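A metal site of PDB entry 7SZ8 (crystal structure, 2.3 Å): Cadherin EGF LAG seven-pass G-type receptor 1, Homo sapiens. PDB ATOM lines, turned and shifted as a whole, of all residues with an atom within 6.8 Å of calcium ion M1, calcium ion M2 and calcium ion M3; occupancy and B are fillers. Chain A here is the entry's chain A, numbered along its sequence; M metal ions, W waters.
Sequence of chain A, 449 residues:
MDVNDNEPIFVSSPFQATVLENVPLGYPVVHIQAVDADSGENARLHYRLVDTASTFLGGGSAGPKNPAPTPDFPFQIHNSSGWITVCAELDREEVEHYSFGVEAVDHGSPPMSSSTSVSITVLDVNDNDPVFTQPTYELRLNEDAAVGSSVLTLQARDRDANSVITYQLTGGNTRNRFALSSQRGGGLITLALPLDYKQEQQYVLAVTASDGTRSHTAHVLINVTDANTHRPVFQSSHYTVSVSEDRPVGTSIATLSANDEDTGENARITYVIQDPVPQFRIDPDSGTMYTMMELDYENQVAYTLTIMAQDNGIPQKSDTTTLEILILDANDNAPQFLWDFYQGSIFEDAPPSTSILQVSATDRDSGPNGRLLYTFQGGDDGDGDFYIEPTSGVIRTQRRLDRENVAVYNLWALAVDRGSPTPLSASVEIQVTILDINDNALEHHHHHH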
ATOM      1  N   GLU A 245      32.735  23.019  -0.773  1.00  0.00           N
ATOM      2  CA  GLU A 245      32.708  23.074   0.715  1.00  0.00           C
ATOM      3  C   GLU A 245      33.993  22.433   1.303  1.00  0.00           C
ATOM      4  O   GLU A 245      34.251  22.638   2.513  1.00  0.00           O
ATOM      5  CB  GLU A 245      31.405  22.458   1.199  1.00  0.00           C
ATOM      6  CG  GLU A 245      31.400  20.949   1.106  1.00  0.00           C
ATOM      7  CD  GLU A 245      30.206  20.318   1.789  1.00  0.00           C
ATOM      8  OE1 GLU A 245      29.555  19.458   1.156  1.00  0.00           O
ATOM      9  OE2 GLU A 245      29.936  20.681   2.955  1.00  0.00           O
ATOM     10  N   LEU A 295      33.797  25.984   5.264  1.00  0.00           N
ATOM     11  CA  LEU A 295      32.456  26.166   4.641  1.00  0.00           C
ATOM     12  C   LEU A 295      31.698  24.850   4.753  1.00  0.00           C
ATOM     13  O   LEU A 295      32.379  23.811   4.678  1.00  0.00           O
ATOM     14  CB  LEU A 295      32.653  26.557   3.179  1.00  0.00           C
ATOM     15  CG  LEU A 295      33.341  27.902   2.994  1.00  0.00           C
ATOM     16  CD1 LEU A 295      33.801  28.117   1.546  1.00  0.00           C
ATOM     17  CD2 LEU A 295      32.424  29.018   3.468  1.00  0.00           C
ATOM     18  N   ASP A 296      30.379  24.890   4.941  1.00  0.00           N
ATOM     19  CA  ASP A 296      29.549  23.654   5.009  1.00  0.00           C
ATOM     20  C   ASP A 296      28.304  23.819   4.145  1.00  0.00           C
ATOM     21  O   ASP A 296      27.359  24.531   4.557  1.00  0.00           O
ATOM     22  CB  ASP A 296      29.207  23.259   6.443  1.00  0.00           C
ATOM     23  CG  ASP A 296      28.444  21.941   6.645  1.00  0.00           C
ATOM     24  OD1 ASP A 296      28.038  21.291   5.653  1.00  0.00           O
ATOM     25  OD2 ASP A 296      28.208  21.593   7.816  1.00  0.00           O
ATOM     26  N   TYR A 297      28.288  23.121   3.014  1.00  0.00           N
ATOM     27  CA  TYR A 297      27.110  23.040   2.123  1.00  0.00           C
ATOM     28  C   TYR A 297      25.846  22.689   2.913  1.00  0.00           C
ATOM     29  O   TYR A 297      24.771  23.228   2.571  1.00  0.00           O
ATOM     30  CB  TYR A 297      27.327  22.038   0.986  1.00  0.00           C
ATOM     31  CG  TYR A 297      26.215  22.024  -0.018  1.00  0.00           C
ATOM     32  CD1 TYR A 297      25.114  21.213   0.186  1.00  0.00           C
ATOM     33  CD2 TYR A 297      26.237  22.828  -1.145  1.00  0.00           C
ATOM     34  CE1 TYR A 297      24.067  21.192  -0.715  1.00  0.00           C
ATOM     35  CE2 TYR A 297      25.206  22.806  -2.069  1.00  0.00           C
ATOM     36  CZ  TYR A 297      24.115  21.980  -1.849  1.00  0.00           C
ATOM     37  OH  TYR A 297      23.059  21.923  -2.729  1.00  0.00           O
ATOM     38  N   GLU A 298      25.939  21.786   3.909  1.00  0.00           N
ATOM     39  CA  GLU A 298      24.745  21.296   4.669  1.00  0.00           C
ATOM     40  C   GLU A 298      24.205  22.393   5.605  1.00  0.00           C
ATOM     41  O   GLU A 298      23.128  22.192   6.171  1.00  0.00           O
ATOM     42  CB  GLU A 298      25.072  20.010   5.435  1.00  0.00           C
ATOM     43  CG  GLU A 298      25.159  18.764   4.540  1.00  0.00           C
ATOM     44  CD  GLU A 298      26.202  18.782   3.420  1.00  0.00           C
ATOM     45  OE1 GLU A 298      27.415  18.870   3.707  1.00  0.00           O
ATOM     46  OE2 GLU A 298      25.807  18.691   2.283  1.00  0.00           O
ATOM     47  N   ASN A 299      24.917  23.513   5.729  1.00  0.00           N
ATOM     48  CA  ASN A 299      24.585  24.648   6.630  1.00  0.00           C
ATOM     49  C   ASN A 299      24.160  25.917   5.851  1.00  0.00           C
ATOM     50  O   ASN A 299      23.136  26.511   6.252  1.00  0.00           O
ATOM     51  CB  ASN A 299      25.747  24.949   7.565  1.00  0.00           C
ATOM     52  CG  ASN A 299      25.465  26.161   8.410  1.00  0.00           C
ATOM     53  OD1 ASN A 299      26.155  27.160   8.297  1.00  0.00           O
ATOM     54  ND2 ASN A 299      24.411  26.081   9.213  1.00  0.00           N
ATOM     55  N   LEU A 328      29.627  24.393  -3.514  1.00  0.00           N
ATOM     56  CA  LEU A 328      29.427  23.072  -4.161  1.00  0.00           C
ATOM     57  C   LEU A 328      29.544  21.980  -3.104  1.00  0.00           C
ATOM     58  O   LEU A 328      30.527  21.984  -2.311  1.00  0.00           O
ATOM     59  CB  LEU A 328      30.437  22.860  -5.281  1.00  0.00           C
ATOM     60  CG  LEU A 328      30.384  23.863  -6.434  1.00  0.00           C
ATOM     61  CD1 LEU A 328      31.282  23.396  -7.553  1.00  0.00           C
ATOM     62  CD2 LEU A 328      28.977  24.098  -6.952  1.00  0.00           C
ATOM     63  N   ASP A 329      28.552  21.100  -3.061  1.00  0.00           N
ATOM     64  CA  ASP A 329      28.482  19.961  -2.116  1.00  0.00           C
ATOM     65  C   ASP A 329      29.640  18.984  -2.389  1.00  0.00           C
ATOM     66  O   ASP A 329      29.970  18.759  -3.532  1.00  0.00           O
ATOM     67  CB  ASP A 329      27.097  19.301  -2.176  1.00  0.00           C
ATOM     68  CG  ASP A 329      26.939  18.082  -1.293  1.00  0.00           C
ATOM     69  OD1 ASP A 329      27.344  18.136  -0.105  1.00  0.00           O
ATOM     70  OD2 ASP A 329      26.400  17.078  -1.817  1.00  0.00           O
ATOM     71  N   ALA A 330      30.217  18.450  -1.324  1.00  0.00           N
ATOM     72  CA  ALA A 330      31.304  17.456  -1.312  1.00  0.00           C
ATOM     73  C   ALA A 330      30.776  16.211  -0.569  1.00  0.00           C
ATOM     74  O   ALA A 330      29.904  16.362   0.297  1.00  0.00           O
ATOM     75  CB  ALA A 330      32.483  18.103  -0.616  1.00  0.00           C
ATOM     76  N   ASN A 331      31.287  15.014  -0.883  1.00  0.00           N
ATOM     77  CA  ASN A 331      30.801  13.778  -0.215  1.00  0.00           C
ATOM     78  C   ASN A 331      31.447  13.697   1.174  1.00  0.00           C
ATOM     79  O   ASN A 331      32.317  12.853   1.399  1.00  0.00           O
ATOM     80  CB  ASN A 331      31.034  12.516  -1.047  1.00  0.00           C
ATOM     81  CG  ASN A 331      30.182  11.349  -0.573  1.00  0.00           C
ATOM     82  OD1 ASN A 331      29.101  11.529   0.001  1.00  0.00           O
ATOM     83  ND2 ASN A 331      30.685  10.144  -0.789  1.00  0.00           N
ATOM     84  N   ASP A 332      31.018  14.556   2.087  1.00  0.00           N
ATOM     85  CA  ASP A 332      31.574  14.582   3.461  1.00  0.00           C
ATOM     86  C   ASP A 332      30.509  14.071   4.434  1.00  0.00           C
ATOM     87  O   ASP A 332      30.620  14.355   5.619  1.00  0.00           O
ATOM     88  CB  ASP A 332      32.144  15.977   3.789  1.00  0.00           C
ATOM     89  CG  ASP A 332      31.145  17.128   3.783  1.00  0.00           C
ATOM     90  OD1 ASP A 332      29.914  16.898   3.468  1.00  0.00           O
ATOM     91  OD2 ASP A 332      31.603  18.261   4.078  1.00  0.00           O
ATOM     92  N   ASN A 333      29.526  13.291   3.968  1.00  0.00           N
ATOM     93  CA  ASN A 333      28.589  12.605   4.908  1.00  0.00           C
ATOM     94  C   ASN A 333      28.426  11.153   4.480  1.00  0.00           C
ATOM     95  O   ASN A 333      28.174  10.911   3.268  1.00  0.00           O
ATOM     96  CB  ASN A 333      27.230  13.311   5.014  1.00  0.00           C
ATOM     97  CG  ASN A 333      27.312  14.600   5.790  1.00  0.00           C
ATOM     98  OD1 ASN A 333      27.110  14.585   7.005  1.00  0.00           O
ATOM     99  ND2 ASN A 333      27.641  15.704   5.144  1.00  0.00           N
ATOM    100  N   ALA A 334      28.520  10.253   5.451  1.00  0.00           N
ATOM    101  CA  ALA A 334      28.381   8.786   5.319  1.00  0.00           C
ATOM    102  C   ALA A 334      26.913   8.445   5.499  1.00  0.00           C
ATOM    103  O   ALA A 334      26.273   8.987   6.377  1.00  0.00           O
ATOM    104  CB  ALA A 334      29.235   8.055   6.332  1.00  0.00           C
ATOM    105  N   PRO A 335      26.334   7.512   4.706  1.00  0.00           N
ATOM    106  CA  PRO A 335      24.983   7.044   4.996  1.00  0.00           C
ATOM    107  C   PRO A 335      24.847   6.569   6.444  1.00  0.00           C
ATOM    108  O   PRO A 335      25.855   6.243   7.077  1.00  0.00           O
ATOM    109  CB  PRO A 335      24.783   5.938   3.972  1.00  0.00           C
ATOM    110  CG  PRO A 335      25.667   6.377   2.815  1.00  0.00           C
ATOM    111  CD  PRO A 335      26.910   6.897   3.502  1.00  0.00           C
ATOM    112  N   ASP A 363      21.360  10.227   4.099  1.00  0.00           N
ATOM    113  CA  ASP A 363      22.674  10.832   3.768  1.00  0.00           C
ATOM    114  C   ASP A 363      22.405  12.326   3.622  1.00  0.00           C
ATOM    115  O   ASP A 363      21.562  12.712   2.763  1.00  0.00           O
ATOM    116  CB  ASP A 363      23.325  10.166   2.541  1.00  0.00           C
ATOM    117  CG  ASP A 363      24.698  10.707   2.184  1.00  0.00           C
ATOM    118  OD1 ASP A 363      24.932  11.922   2.411  1.00  0.00           O
ATOM    119  OD2 ASP A 363      25.556   9.908   1.652  1.00  0.00           O
ATOM    120  N   ARG A 364      23.114  13.132   4.423  1.00  0.00           N
ATOM    121  CA  ARG A 364      22.833  14.583   4.568  1.00  0.00           C
ATOM    122  C   ARG A 364      23.294  15.334   3.310  1.00  0.00           C
ATOM    123  O   ARG A 364      22.782  16.424   3.061  1.00  0.00           O
ATOM    124  CB  ARG A 364      23.445  15.102   5.873  1.00  0.00           C
ATOM    125  CG  ARG A 364      22.914  14.418   7.115  1.00  0.00           C
ATOM    126  CD  ARG A 364      23.668  14.956   8.301  1.00  0.00           C
ATOM    127  NE  ARG A 364      23.435  16.395   8.461  1.00  0.00           N
ATOM    128  CZ  ARG A 364      24.357  17.359   8.326  1.00  0.00           C
ATOM    129  NH1 ARG A 364      25.608  17.067   8.006  1.00  0.00           N
ATOM    130  NH2 ARG A 364      24.014  18.623   8.526  1.00  0.00           N
ATOM    131  N   ASP A 365      24.162  14.725   2.502  1.00  0.00           N
ATOM    132  CA  ASP A 365      24.631  15.252   1.194  1.00  0.00           C
ATOM    133  C   ASP A 365      23.460  15.299   0.199  1.00  0.00           C
ATOM    134  O   ASP A 365      22.422  14.633   0.419  1.00  0.00           O
ATOM    135  CB  ASP A 365      25.815  14.418   0.675  1.00  0.00           C
ATOM    136  CG  ASP A 365      27.056  14.489   1.574  1.00  0.00           C
ATOM    137  OD1 ASP A 365      27.422  15.607   2.004  1.00  0.00           O
ATOM    138  OD2 ASP A 365      27.640  13.429   1.826  1.00  0.00           O
ATOM    139  N   SER A 366      23.629  16.059  -0.888  1.00  0.00           N
ATOM    140  CA  SER A 366      22.660  16.185  -2.018  1.00  0.00           C
ATOM    141  C   SER A 366      23.276  15.547  -3.270  1.00  0.00           C
ATOM    142  O   SER A 366      24.481  15.177  -3.217  1.00  0.00           O
ATOM    143  CB  SER A 366      22.293  17.644  -2.244  1.00  0.00           C
ATOM    144  OG  SER A 366      22.165  18.342  -1.004  1.00  0.00           O
ATOM    145  N   PRO A 368      24.309  12.979  -6.422  1.00  0.00           N
ATOM    146  CA  PRO A 368      25.003  11.688  -6.253  1.00  0.00           C
ATOM    147  C   PRO A 368      25.577  11.431  -4.843  1.00  0.00           C
ATOM    148  O   PRO A 368      25.551  10.278  -4.359  1.00  0.00           O
ATOM    149  CB  PRO A 368      26.135  11.760  -7.293  1.00  0.00           C
ATOM    150  CG  PRO A 368      25.620  12.700  -8.391  1.00  0.00           C
ATOM    151  CD  PRO A 368      24.704  13.667  -7.670  1.00  0.00           C
ATOM    152  N   ASN A 369      26.039  12.487  -4.176  1.00  0.00           N
ATOM    153  CA  ASN A 369      26.636  12.374  -2.827  1.00  0.00           C
ATOM    154  C   ASN A 369      25.591  11.823  -1.855  1.00  0.00           C
ATOM    155  O   ASN A 369      25.981  11.127  -0.878  1.00  0.00           O
ATOM    156  CB  ASN A 369      27.230  13.712  -2.395  1.00  0.00           C
ATOM    157  CG  ASN A 369      28.340  14.183  -3.310  1.00  0.00           C
ATOM    158  OD1 ASN A 369      29.103  13.356  -3.811  1.00  0.00           O
ATOM    159  ND2 ASN A 369      28.436  15.475  -3.544  1.00  0.00           N
ATOM    160  N   GLY A 370      24.311  12.143  -2.073  1.00  0.00           N
ATOM    161  CA  GLY A 370      23.191  11.846  -1.149  1.00  0.00           C
ATOM    162  C   GLY A 370      22.345  10.648  -1.568  1.00  0.00           C
ATOM    163  O   GLY A 370      21.558  10.204  -0.721  1.00  0.00           O
ATOM    164  N   ARG A 371      22.528  10.151  -2.800  1.00  0.00           N
ATOM    165  CA  ARG A 371      21.744   9.063  -3.456  1.00  0.00           C
ATOM    166  C   ARG A 371      22.316   7.665  -3.116  1.00  0.00           C
ATOM    167  O   ARG A 371      23.511   7.449  -3.282  1.00  0.00           O
ATOM    168  CB  ARG A 371      21.776   9.270  -4.965  1.00  0.00           C
ATOM    169  CG  ARG A 371      20.715   8.490  -5.729  1.00  0.00           C
ATOM    170  CD  ARG A 371      20.732   8.891  -7.175  1.00  0.00           C
ATOM    171  NE  ARG A 371      20.358   7.768  -8.033  1.00  0.00           N
ATOM    172  CZ  ARG A 371      20.600   7.681  -9.336  1.00  0.00           C
ATOM    173  NH1 ARG A 371      21.235   8.665  -9.976  1.00  0.00           N
ATOM    174  NH2 ARG A 371      20.196   6.625 -10.015  1.00  0.00           N
ATOM    175  N   LEU A 372      21.452   6.724  -2.748  1.00  0.00           N
ATOM    176  CA  LEU A 372      21.808   5.501  -1.975  1.00  0.00           C
ATOM    177  C   LEU A 372      21.574   4.210  -2.791  1.00  0.00           C
ATOM    178  O   LEU A 372      20.572   4.109  -3.522  1.00  0.00           O
ATOM    179  CB  LEU A 372      21.010   5.545  -0.664  1.00  0.00           C
ATOM    180  CG  LEU A 372      21.441   6.658   0.293  1.00  0.00           C
ATOM    181  CD1 LEU A 372      20.506   6.800   1.466  1.00  0.00           C
ATOM    182  CD2 LEU A 372      22.860   6.434   0.783  1.00  0.00           C
ATOM    183  N   ASP A 417      26.545   5.564  -0.874  1.00  0.00           N
ATOM    184  CA  ASP A 417      26.220   6.745  -1.726  1.00  0.00           C
ATOM    185  C   ASP A 417      26.949   6.589  -3.068  1.00  0.00           C
ATOM    186  O   ASP A 417      27.825   5.722  -3.177  1.00  0.00           O
ATOM    187  CB  ASP A 417      26.531   8.064  -1.014  1.00  0.00           C
ATOM    188  CG  ASP A 417      27.965   8.288  -0.573  1.00  0.00           C
ATOM    189  OD1 ASP A 417      28.934   7.896  -1.336  1.00  0.00           O
ATOM    190  OD2 ASP A 417      28.129   8.865   0.535  1.00  0.00           O
ATOM    191  N   ARG A 418      26.609   7.440  -4.037  1.00  0.00           N
ATOM    192  CA  ARG A 418      27.252   7.501  -5.381  1.00  0.00           C
ATOM    193  C   ARG A 418      28.208   8.708  -5.466  1.00  0.00           C
ATOM    194  O   ARG A 418      28.247   9.358  -6.505  1.00  0.00           O
ATOM    195  CB  ARG A 418      26.157   7.607  -6.439  1.00  0.00           C
ATOM    196  CG  ARG A 418      24.920   6.766  -6.137  1.00  0.00           C
ATOM    197  CD  ARG A 418      25.204   5.325  -5.772  1.00  0.00           C
ATOM    198  NE  ARG A 418      23.944   4.604  -5.864  1.00  0.00           N
ATOM    199  CZ  ARG A 418      23.434   4.062  -6.992  1.00  0.00           C
ATOM    200  NH1 ARG A 418      24.111   4.102  -8.133  1.00  0.00           N
ATOM    201  NH2 ARG A 418      22.261   3.463  -6.949  1.00  0.00           N
ATOM    202  N   GLY A 419      28.952   8.993  -4.399  1.00  0.00           N
ATOM    203  CA  GLY A 419      29.840  10.166  -4.332  1.00  0.00           C
ATOM    204  C   GLY A 419      31.089   9.928  -5.149  1.00  0.00           C
ATOM    205  O   GLY A 419      31.662   8.820  -5.044  1.00  0.00           O
ATOM    206  N   LEU A 424      31.097   6.837  -0.026  1.00  0.00           N
ATOM    207  CA  LEU A 424      31.014   6.463   1.425  1.00  0.00           C
ATOM    208  C   LEU A 424      29.910   5.426   1.640  1.00  0.00           C
ATOM    209  O   LEU A 424      28.989   5.369   0.808  1.00  0.00           O
ATOM    210  CB  LEU A 424      30.772   7.672   2.331  1.00  0.00           C
ATOM    211  CG  LEU A 424      31.949   8.622   2.525  1.00  0.00           C
ATOM    212  CD1 LEU A 424      31.481   9.981   3.035  1.00  0.00           C
ATOM    213  CD2 LEU A 424      33.001   8.031   3.465  1.00  0.00           C
HETATM  214 CA    CA M   1      28.264  17.585   1.797  1.00  0.00          CA
HETATM  215 CA    CA M   2      29.517  19.513   4.935  1.00  0.00          CA
HETATM  216 CA    CA M   3      27.224  11.085   1.207  1.00  0.00          CA
HETATM  217  O   HOH W   1      30.970  20.521   5.918  1.00  0.00           O
HETATM  218  O   HOH W   2      29.137  18.222   6.482  1.00  0.00           O
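The side-chain carboxylate of Asp 417 lies within hydrogen-bond range of the backbone NH of Leu 424, 2.7 Å away. ND2 of Asn 333 lies close to OD1 of Asp 332, at 3.1 Å. The guanidinium group (NH1) of Arg 364 sits at hydrogen-bond distance from the side-chain amide oxygen (OD1) of Asn 333. The side-chain carboxylate (OD2) of Asp 329 lies within hydrogen-bond range of the side-chain amide nitrogen (ND2) of Asn 369 (3.1 Å). N of Leu 424 lies close to ND2 of Asn 331 (3.4 Å). The side-chain carboxylate of Glu 245 lies close to the backbone NH of Tyr 297 (2.9 Å). The side-chain carboxylate (OD1) of Asp 417 is in hydrogen-bond range of the backbone NH (N) of Gly 419. O of Leu 328 is in hydrogen-bond range of N of Glu 245 (2.9 Å).
Seven residues have an atom within 4 Å of calcium ion M1: Glu 245, Glu 298, Asp 329, Ala 330, Asp 332, Asn 333 and Asp 365. The nearest printed residue that does not touch calcium ion M1 is Tyr 297 (4.6 Å).
Of the 27 residues printed, 4 come within 4 Å of calcium ion M2. Along chain A the residues within 4 Å of calcium ion M2 span positions 245 to 332.
Of the 27 residues printed, 6 come within 4 Å of calcium ion M3. The nearest printed residue that does not touch calcium ion M3 is Gly 370 (4.5 Å).
Calcium ion M1 is bound by OD1 of Asp 365 (2.2 Å). Calcium ion M1 is bound by the side-chain carboxylate (OD1) of Asp 329, 2.2 Å away. The side-chain carboxylate (OE1) of Glu 245 binds calcium ion M1. OD1 of Asp 332 is bound to calcium ion M1, at 2.4 Å. The side-chain carboxylate (OE1) of Glu 298 is bound to calcium ion M1 (2.5 Å). O of Ala 330 binds calcium ion M1 (2.5 Å). OE2 of Glu 298 is bound to calcium ion M1, 2.7 Å away. Calcium ion M1 has seven donor atoms within binding distance.
Calcium ion M2 is bound by water W1 (2.0 Å), water W2 (2.1 Å), the side-chain carboxylate of Glu 245 (2.3 Å), the side-chain carboxylate of Asp 296 (2.4 Å), the side-chain carboxylate of Glu 298 (2.5 Å) and the side-chain carboxylate of Asp 332 (2.6 Å). Slightly farther from calcium ion M2 lies OD1 of Asp 332 (3.0 Å).
Calcium ion M3 is bound by OD2 of Asp 363 (2.1 Å), OD1 of Asn 331 (2.3 Å), O of Asn 333 (2.3 Å), O of Asn 369 (2.4 Å), OD2 of Asp 365 (2.5 Å), OD2 of Asp 417 (2.5 Å) and OD1 of Asp 363 (2.7 Å). Calcium ion M3 has seven donor atoms within binding distance.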
